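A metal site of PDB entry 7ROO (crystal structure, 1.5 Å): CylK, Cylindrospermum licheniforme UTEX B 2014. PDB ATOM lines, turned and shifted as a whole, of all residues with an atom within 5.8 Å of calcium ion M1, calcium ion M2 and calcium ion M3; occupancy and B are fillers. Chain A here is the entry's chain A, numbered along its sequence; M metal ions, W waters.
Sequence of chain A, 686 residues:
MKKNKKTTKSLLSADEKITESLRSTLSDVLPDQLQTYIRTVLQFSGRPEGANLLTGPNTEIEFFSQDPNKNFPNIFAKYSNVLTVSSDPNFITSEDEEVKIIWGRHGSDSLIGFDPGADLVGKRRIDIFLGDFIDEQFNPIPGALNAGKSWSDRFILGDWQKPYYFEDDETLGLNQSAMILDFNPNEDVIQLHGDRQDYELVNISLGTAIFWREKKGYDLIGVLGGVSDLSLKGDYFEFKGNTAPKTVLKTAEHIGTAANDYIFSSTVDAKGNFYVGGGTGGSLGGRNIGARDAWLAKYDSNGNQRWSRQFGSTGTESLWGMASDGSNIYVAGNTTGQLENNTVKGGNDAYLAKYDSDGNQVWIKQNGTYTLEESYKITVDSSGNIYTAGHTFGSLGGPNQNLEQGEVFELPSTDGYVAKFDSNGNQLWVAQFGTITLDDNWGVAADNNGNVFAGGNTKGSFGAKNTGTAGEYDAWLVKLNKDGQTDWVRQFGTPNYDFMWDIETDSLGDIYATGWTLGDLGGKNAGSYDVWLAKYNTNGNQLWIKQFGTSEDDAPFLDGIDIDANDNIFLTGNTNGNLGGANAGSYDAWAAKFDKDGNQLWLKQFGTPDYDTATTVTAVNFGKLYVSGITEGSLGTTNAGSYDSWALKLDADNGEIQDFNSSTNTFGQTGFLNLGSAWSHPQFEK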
ATOM      1  N   LEU A  83       7.022  32.581  -3.710  1.00  0.00           N
ATOM      2  CA  LEU A  83       7.346  31.242  -3.211  1.00  0.00           C
ATOM      3  C   LEU A  83       8.543  30.715  -3.980  1.00  0.00           C
ATOM      4  O   LEU A  83       9.279  31.547  -4.550  1.00  0.00           O
ATOM      5  CB  LEU A  83       6.098  30.388  -3.315  1.00  0.00           C
ATOM      6  CG  LEU A  83       4.999  30.802  -2.327  1.00  0.00           C
ATOM      7  CD1 LEU A  83       3.662  30.244  -2.716  1.00  0.00           C
ATOM      8  CD2 LEU A  83       5.412  30.418  -0.910  1.00  0.00           C
ATOM      9  N   THR A  84       8.775  29.410  -3.953  1.00  0.00           N
ATOM     10  CA  THR A  84      10.095  28.863  -4.346  1.00  0.00           C
ATOM     11  C   THR A  84       9.995  28.059  -5.633  1.00  0.00           C
ATOM     12  O   THR A  84       8.955  27.942  -6.193  1.00  0.00           O
ATOM     13  CB  THR A  84      10.719  28.008  -3.231  1.00  0.00           C
ATOM     14  OG1 THR A  84      10.168  26.700  -3.272  1.00  0.00           O
ATOM     15  CG2 THR A  84      10.585  28.644  -1.868  1.00  0.00           C
ATOM     16  N   VAL A  85      11.121  27.581  -6.104  1.00  0.00           N
ATOM     17  CA  VAL A  85      11.182  26.705  -7.291  1.00  0.00           C
ATOM     18  C   VAL A  85      10.558  25.359  -6.960  1.00  0.00           C
ATOM     19  O   VAL A  85      10.319  24.547  -7.916  1.00  0.00           O
ATOM     20  CB  VAL A  85      12.607  26.629  -7.846  1.00  0.00           C
ATOM     21  CG1 VAL A  85      12.711  25.853  -9.131  1.00  0.00           C
ATOM     22  CG2 VAL A  85      13.171  28.003  -8.063  1.00  0.00           C
ATOM     23  N   SER A  86      10.318  25.084  -5.670  1.00  0.00           N
ATOM     24  CA  SER A  86       9.722  23.801  -5.215  1.00  0.00           C
ATOM     25  C   SER A  86       8.217  23.747  -5.520  1.00  0.00           C
ATOM     26  O   SER A  86       7.592  24.809  -5.739  1.00  0.00           O
ATOM     27  CB  SER A  86       9.891  23.604  -3.717  1.00  0.00           C
ATOM     28  OG  SER A  86      11.151  24.089  -3.204  1.00  0.00           O
ATOM     29  N   SER A  87       7.570  22.592  -5.391  1.00  0.00           N
ATOM     30  CA  SER A  87       6.093  22.489  -5.267  1.00  0.00           C
ATOM     31  C   SER A  87       5.705  22.926  -3.846  1.00  0.00           C
ATOM     32  O   SER A  87       5.870  22.199  -2.907  1.00  0.00           O
ATOM     33  CB  SER A  87       5.644  21.095  -5.583  1.00  0.00           C
ATOM     34  OG  SER A  87       6.052  20.793  -6.916  1.00  0.00           O
ATOM     35  N   ASP A  88       5.251  24.157  -3.711  1.00  0.00           N
ATOM     36  CA  ASP A  88       5.084  24.837  -2.409  1.00  0.00           C
ATOM     37  C   ASP A  88       3.629  24.841  -1.981  1.00  0.00           C
ATOM     38  O   ASP A  88       2.744  25.259  -2.745  1.00  0.00           O
ATOM     39  CB  ASP A  88       5.478  26.299  -2.504  1.00  0.00           C
ATOM     40  CG  ASP A  88       6.911  26.536  -2.943  1.00  0.00           C
ATOM     41  OD1 ASP A  88       7.847  26.195  -2.199  1.00  0.00           O
ATOM     42  OD2 ASP A  88       6.998  27.173  -4.008  1.00  0.00           O
ATOM     43  N   GLY A 104       3.464  31.501  -7.219  1.00  0.00           N
ATOM     44  CA  GLY A 104       3.970  30.140  -6.974  1.00  0.00           C
ATOM     45  C   GLY A 104       5.322  29.844  -7.602  1.00  0.00           C
ATOM     46  O   GLY A 104       6.112  29.032  -7.062  1.00  0.00           O
ATOM     47  N   ARG A 105       5.578  30.404  -8.768  1.00  0.00           N
ATOM     48  CA  ARG A 105       6.802  30.100  -9.553  1.00  0.00           C
ATOM     49  C   ARG A 105       6.788  28.612  -9.887  1.00  0.00           C
ATOM     50  O   ARG A 105       5.749  28.057 -10.028  1.00  0.00           O
ATOM     51  CB  ARG A 105       8.094  30.589  -8.883  1.00  0.00           C
ATOM     52  CG  ARG A 105       8.162  32.103  -8.807  1.00  0.00           C
ATOM     53  CD  ARG A 105       9.300  32.682  -8.027  1.00  0.00           C
ATOM     54  NE  ARG A 105      10.636  32.305  -8.513  1.00  0.00           N
ATOM     55  CZ  ARG A 105      11.636  31.826  -7.786  1.00  0.00           C
ATOM     56  NH1 ARG A 105      11.486  31.498  -6.512  1.00  0.00           N
ATOM     57  NH2 ARG A 105      12.807  31.629  -8.361  1.00  0.00           N
ATOM     58  N   HIS A 106       7.941  28.018 -10.103  1.00  0.00           N
ATOM     59  CA  HIS A 106       7.965  26.622 -10.616  1.00  0.00           C
ATOM     60  C   HIS A 106       7.301  25.691  -9.595  1.00  0.00           C
ATOM     61  O   HIS A 106       7.222  26.032  -8.415  1.00  0.00           O
ATOM     62  CB  HIS A 106       9.405  26.155 -10.889  1.00  0.00           C
ATOM     63  CG  HIS A 106      10.286  27.199 -11.498  1.00  0.00           C
ATOM     64  ND1 HIS A 106      10.584  28.363 -10.793  1.00  0.00           N
ATOM     65  CD2 HIS A 106      10.998  27.244 -12.664  1.00  0.00           C
ATOM     66  CE1 HIS A 106      11.430  29.097 -11.541  1.00  0.00           C
ATOM     67  NE2 HIS A 106      11.695  28.408 -12.661  1.00  0.00           N
ATOM     68  N   GLY A 107       7.027  24.477 -10.019  1.00  0.00           N
ATOM     69  CA  GLY A 107       6.425  23.461  -9.134  1.00  0.00           C
ATOM     70  C   GLY A 107       4.912  23.546  -9.122  1.00  0.00           C
ATOM     71  O   GLY A 107       4.293  24.502  -9.583  1.00  0.00           O
ATOM     72  N   SER A 108       4.323  22.451  -8.646  1.00  0.00           N
ATOM     73  CA  SER A 108       2.884  22.269  -8.459  1.00  0.00           C
ATOM     74  C   SER A 108       2.462  22.876  -7.134  1.00  0.00           C
ATOM     75  O   SER A 108       2.634  22.215  -6.121  1.00  0.00           O
ATOM     76  CB  SER A 108       2.595  20.815  -8.476  1.00  0.00           C
ATOM     77  OG  SER A 108       3.010  20.290  -9.708  1.00  0.00           O
ATOM     78  N   ASP A 109       2.083  24.144  -7.115  1.00  0.00           N
ATOM     79  CA  ASP A 109       1.914  24.878  -5.862  1.00  0.00           C
ATOM     80  C   ASP A 109       0.468  24.761  -5.387  1.00  0.00           C
ATOM     81  O   ASP A 109      -0.461  24.750  -6.213  1.00  0.00           O
ATOM     82  CB  ASP A 109       2.320  26.313  -6.051  1.00  0.00           C
ATOM     83  CG  ASP A 109       3.753  26.434  -6.528  1.00  0.00           C
ATOM     84  OD1 ASP A 109       4.662  26.037  -5.797  1.00  0.00           O
ATOM     85  OD2 ASP A 109       3.943  26.960  -7.637  1.00  0.00           O
ATOM     86  N   LEU A 130      -0.711  34.045  -9.134  1.00  0.00           N
ATOM     87  CA  LEU A 130       0.112  33.619 -10.282  1.00  0.00           C
ATOM     88  C   LEU A 130       0.552  32.205  -9.964  1.00  0.00           C
ATOM     89  O   LEU A 130       1.496  32.043  -9.179  1.00  0.00           O
ATOM     90  CB  LEU A 130       1.320  34.542 -10.423  1.00  0.00           C
ATOM     91  CG  LEU A 130       1.046  36.044 -10.607  1.00  0.00           C
ATOM     92  CD1 LEU A 130       2.372  36.777 -10.765  1.00  0.00           C
ATOM     93  CD2 LEU A 130       0.176  36.268 -11.793  1.00  0.00           C
ATOM     94  N   GLY A 131      -0.059  31.198 -10.569  1.00  0.00           N
ATOM     95  CA  GLY A 131       0.338  29.799 -10.293  1.00  0.00           C
ATOM     96  C   GLY A 131       1.783  29.514 -10.656  1.00  0.00           C
ATOM     97  O   GLY A 131       2.493  28.841  -9.868  1.00  0.00           O
ATOM     98  N   ASP A 132       2.191  29.914 -11.874  1.00  0.00           N
ATOM     99  CA  ASP A 132       3.560  29.689 -12.393  1.00  0.00           C
ATOM    100  C   ASP A 132       4.234  31.049 -12.574  1.00  0.00           C
ATOM    101  O   ASP A 132       4.793  31.571 -11.622  1.00  0.00           O
ATOM    102  CB  ASP A 132       3.471  28.758 -13.595  1.00  0.00           C
ATOM    103  CG  ASP A 132       3.256  27.315 -13.265  1.00  0.00           C
ATOM    104  OD1 ASP A 132       3.799  26.826 -12.194  1.00  0.00           O
ATOM    105  OD2 ASP A 132       2.606  26.648 -14.125  1.00  0.00           O
ATOM    106  N   ILE A 134       6.914  31.572 -14.119  1.00  0.00           N
ATOM    107  CA  ILE A 134       8.276  31.141 -13.781  1.00  0.00           C
ATOM    108  C   ILE A 134       9.240  32.186 -14.301  1.00  0.00           C
ATOM    109  O   ILE A 134       8.962  32.908 -15.283  1.00  0.00           O
ATOM    110  CB  ILE A 134       8.608  29.704 -14.203  1.00  0.00           C
ATOM    111  CG1 ILE A 134       8.764  29.563 -15.722  1.00  0.00           C
ATOM    112  CG2 ILE A 134       7.588  28.706 -13.615  1.00  0.00           C
ATOM    113  CD1 ILE A 134       9.200  28.181 -16.162  1.00  0.00           C
ATOM    114  N   SER A 150       5.300  24.235 -17.492  1.00  0.00           N
ATOM    115  CA  SER A 150       4.207  24.660 -16.584  1.00  0.00           C
ATOM    116  C   SER A 150       3.910  23.495 -15.665  1.00  0.00           C
ATOM    117  O   SER A 150       4.199  22.313 -16.020  1.00  0.00           O
ATOM    118  CB  SER A 150       3.013  25.148 -17.327  1.00  0.00           C
ATOM    119  OG  SER A 150       2.426  24.089 -18.102  1.00  0.00           O
ATOM    120  N   TRP A 151       3.262  23.763 -14.533  1.00  0.00           N
ATOM    121  CA  TRP A 151       2.895  22.756 -13.514  1.00  0.00           C
ATOM    122  C   TRP A 151       1.426  22.872 -13.161  1.00  0.00           C
ATOM    123  O   TRP A 151       0.854  23.988 -13.347  1.00  0.00           O
ATOM    124  CB  TRP A 151       3.758  22.930 -12.273  1.00  0.00           C
ATOM    125  CG  TRP A 151       5.194  22.521 -12.398  1.00  0.00           C
ATOM    126  CD1 TRP A 151       5.678  21.320 -11.979  1.00  0.00           C
ATOM    127  CD2 TRP A 151       6.294  23.222 -13.024  1.00  0.00           C
ATOM    128  NE1 TRP A 151       7.023  21.265 -12.219  1.00  0.00           N
ATOM    129  CE2 TRP A 151       7.420  22.401 -12.885  1.00  0.00           C
ATOM    130  CE3 TRP A 151       6.455  24.470 -13.645  1.00  0.00           C
ATOM    131  CZ2 TRP A 151       8.695  22.750 -13.362  1.00  0.00           C
ATOM    132  CZ3 TRP A 151       7.706  24.812 -14.122  1.00  0.00           C
ATOM    133  CH2 TRP A 151       8.804  23.970 -13.974  1.00  0.00           C
ATOM    134  N   SER A 152       0.869  21.810 -12.595  1.00  0.00           N
ATOM    135  CA  SER A 152      -0.515  21.831 -12.059  1.00  0.00           C
ATOM    136  C   SER A 152      -0.541  22.586 -10.734  1.00  0.00           C
ATOM    137  O   SER A 152      -0.024  22.052  -9.726  1.00  0.00           O
ATOM    138  CB  SER A 152      -1.058  20.460 -11.883  1.00  0.00           C
ATOM    139  OG  SER A 152      -2.398  20.537 -11.416  1.00  0.00           O
ATOM    140  N   ASP A 153      -1.058  23.815 -10.746  1.00  0.00           N
ATOM    141  CA  ASP A 153      -1.268  24.605  -9.527  1.00  0.00           C
ATOM    142  C   ASP A 153      -2.688  24.454  -9.036  1.00  0.00           C
ATOM    143  O   ASP A 153      -3.620  24.366  -9.862  1.00  0.00           O
ATOM    144  CB  ASP A 153      -0.869  26.067  -9.723  1.00  0.00           C
ATOM    145  CG  ASP A 153       0.558  26.209 -10.169  1.00  0.00           C
ATOM    146  OD1 ASP A 153       1.497  25.853  -9.368  1.00  0.00           O
ATOM    147  OD2 ASP A 153       0.728  26.728 -11.254  1.00  0.00           O
ATOM    148  N   PHE A 155      -5.516  26.456  -6.801  1.00  0.00           N
ATOM    149  CA  PHE A 155      -5.859  27.776  -6.233  1.00  0.00           C
ATOM    150  C   PHE A 155      -7.001  27.530  -5.235  1.00  0.00           C
ATOM    151  O   PHE A 155      -8.085  27.022  -5.617  1.00  0.00           O
ATOM    152  CB  PHE A 155      -6.311  28.698  -7.369  1.00  0.00           C
ATOM    153  CG  PHE A 155      -5.275  28.887  -8.444  1.00  0.00           C
ATOM    154  CD1 PHE A 155      -4.223  29.784  -8.281  1.00  0.00           C
ATOM    155  CD2 PHE A 155      -5.353  28.168  -9.630  1.00  0.00           C
ATOM    156  CE1 PHE A 155      -3.262  29.950  -9.272  1.00  0.00           C
ATOM    157  CE2 PHE A 155      -4.381  28.326 -10.607  1.00  0.00           C
ATOM    158  CZ  PHE A 155      -3.352  29.244 -10.456  1.00  0.00           C
ATOM    159  N   ASP A 182      -3.335  33.226 -14.271  1.00  0.00           N
ATOM    160  CA  ASP A 182      -2.791  32.254 -15.239  1.00  0.00           C
ATOM    161  C   ASP A 182      -3.456  30.894 -15.063  1.00  0.00           C
ATOM    162  O   ASP A 182      -2.804  29.868 -15.267  1.00  0.00           O
ATOM    163  CB  ASP A 182      -1.268  32.194 -15.161  1.00  0.00           C
ATOM    164  CG  ASP A 182      -0.794  31.580 -13.852  1.00  0.00           C
ATOM    165  OD1 ASP A 182      -1.529  31.694 -12.839  1.00  0.00           O
ATOM    166  OD2 ASP A 182       0.298  30.971 -13.855  1.00  0.00           O
ATOM    167  N   ASN A 184      -4.994  27.652 -16.113  1.00  0.00           N
ATOM    168  CA  ASN A 184      -5.015  26.764 -17.314  1.00  0.00           C
ATOM    169  C   ASN A 184      -5.937  25.589 -17.022  1.00  0.00           C
ATOM    170  O   ASN A 184      -5.554  24.694 -16.271  1.00  0.00           O
ATOM    171  CB  ASN A 184      -3.608  26.356 -17.733  1.00  0.00           C
ATOM    172  CG  ASN A 184      -3.653  25.447 -18.956  1.00  0.00           C
ATOM    173  OD1 ASN A 184      -4.732  25.072 -19.416  1.00  0.00           O
ATOM    174  ND2 ASN A 184      -2.490  25.160 -19.523  1.00  0.00           N
ATOM    175  N   GLU A 187      -4.710  22.006 -16.909  1.00  0.00           N
ATOM    176  CA  GLU A 187      -3.626  21.616 -15.988  1.00  0.00           C
ATOM    177  C   GLU A 187      -3.928  21.974 -14.525  1.00  0.00           C
ATOM    178  O   GLU A 187      -3.617  21.167 -13.616  1.00  0.00           O
ATOM    179  CB  GLU A 187      -2.356  22.341 -16.411  1.00  0.00           C
ATOM    180  CG  GLU A 187      -1.122  21.701 -15.920  1.00  0.00           C
ATOM    181  CD  GLU A 187       0.154  22.110 -16.637  1.00  0.00           C
ATOM    182  OE1 GLU A 187       1.109  21.267 -16.630  1.00  0.00           O
ATOM    183  OE2 GLU A 187       0.245  23.301 -17.047  1.00  0.00           O
ATOM    184  N   ASP A 188      -4.455  23.173 -14.287  1.00  0.00           N
ATOM    185  CA  ASP A 188      -4.597  23.692 -12.903  1.00  0.00           C
ATOM    186  C   ASP A 188      -5.938  23.226 -12.308  1.00  0.00           C
ATOM    187  O   ASP A 188      -6.811  22.670 -13.050  1.00  0.00           O
ATOM    188  CB  ASP A 188      -4.472  25.217 -12.902  1.00  0.00           C
ATOM    189  CG  ASP A 188      -3.158  25.728 -13.438  1.00  0.00           C
ATOM    190  OD1 ASP A 188      -2.158  25.108 -13.147  1.00  0.00           O
ATOM    191  OD2 ASP A 188      -3.142  26.771 -14.110  1.00  0.00           O
HETATM  192 CA    CA M   1       3.606  26.749  -9.954  1.00  0.00          CA
HETATM  193 CA    CA M   2       6.780  26.932  -6.334  1.00  0.00          CA
HETATM  194 CA    CA M   3       0.289  26.186 -13.508  1.00  0.00          CA
HETATM  195  O   HOH W   1      -0.588  28.183 -14.113  1.00  0.00           O
HETATM  196  O   HOH W   2      -0.516  25.530 -15.749  1.00  0.00           O
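Within 4 Å of calcium ion M1: Arg 105, His 106, Gly 107, Asp 109, Gly 131, Asp 132 and Asp 153.
The nearest printed residue that does not touch calcium ion M1 is Gly 104 (4.2 Å).
The backbone NH (N) of Gly 104 lies within hydrogen-bond range of the backbone carbonyl oxygen (O) of Leu 130, at 2.8 Å.
The backbone carbonyl oxygen of Leu 83 sits at hydrogen-bond distance from the guanidinium group of Arg 105, 3.0 Å away.
The backbone NH (N) of Asp 132 is in hydrogen-bond range of the side-chain carboxylate (OD2) of Asp 182, 2.9 Å away.
The side-chain hydroxyl (OG1) of Thr 84 sits at hydrogen-bond distance from the side-chain hydroxyl (OG) of Ser 86 (2.8 Å).
The side-chain carboxylate (OD1) of Asp 182 sits at hydrogen-bond distance from the backbone NH (N) of Gly 131 (2.7 Å).
The side-chain carboxylate (OD2) of Asp 188 lies within hydrogen-bond range of the backbone NH (N) of Asn 184 (2.9 Å).
Of the 25 residues printed, 4 come within 4 Å of calcium ion M3.
Calcium ion M2 is bound by O of His 106, O of Gly 104, OD2 of Asp 88, O of Ser 86, OD1 of Asp 109 and O of Thr 84.
Calcium ion M2 has six donor atoms within binding distance.
Slightly farther from calcium ion M2 lies OD2 of Asp 109 (3.1 Å).
The nearest printed residue that does not touch calcium ion M2 is Val 85 (4.1 Å).
Calcium ion M3 is bound by water W1 (2.3 Å).
Calcium ion M3 is bound by the backbone carbonyl oxygen (O) of Trp 151 (2.3 Å).
OD2 of Asp 153 binds calcium ion M3 (2.4 Å).
OD2 of Asp 132 is bound to calcium ion M3, at 2.4 Å.
Water W2 binds calcium ion M3 (2.5 Å).
OD1 of Asp 188 binds calcium ion M3 (2.7 Å).
Calcium ion M1 is bound by the side-chain carboxylate of Asp 132, the side-chain carboxylate of Asp 109, the side-chain carboxylate of Asp 153, the backbone carbonyl oxygen of Gly 131, the backbone carbonyl oxygen of Gly 107 and the backbone carbonyl oxygen of Arg 105.
Calcium ion M1 has six donor atoms within binding distance.
Water W1 bridges OD2 of Asp 188 and OD2 of Asp 182.
Water W2 bridges OE2 of Glu 187 (2.7 Å) and OD2 of Asp 188 (3.3 Å).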
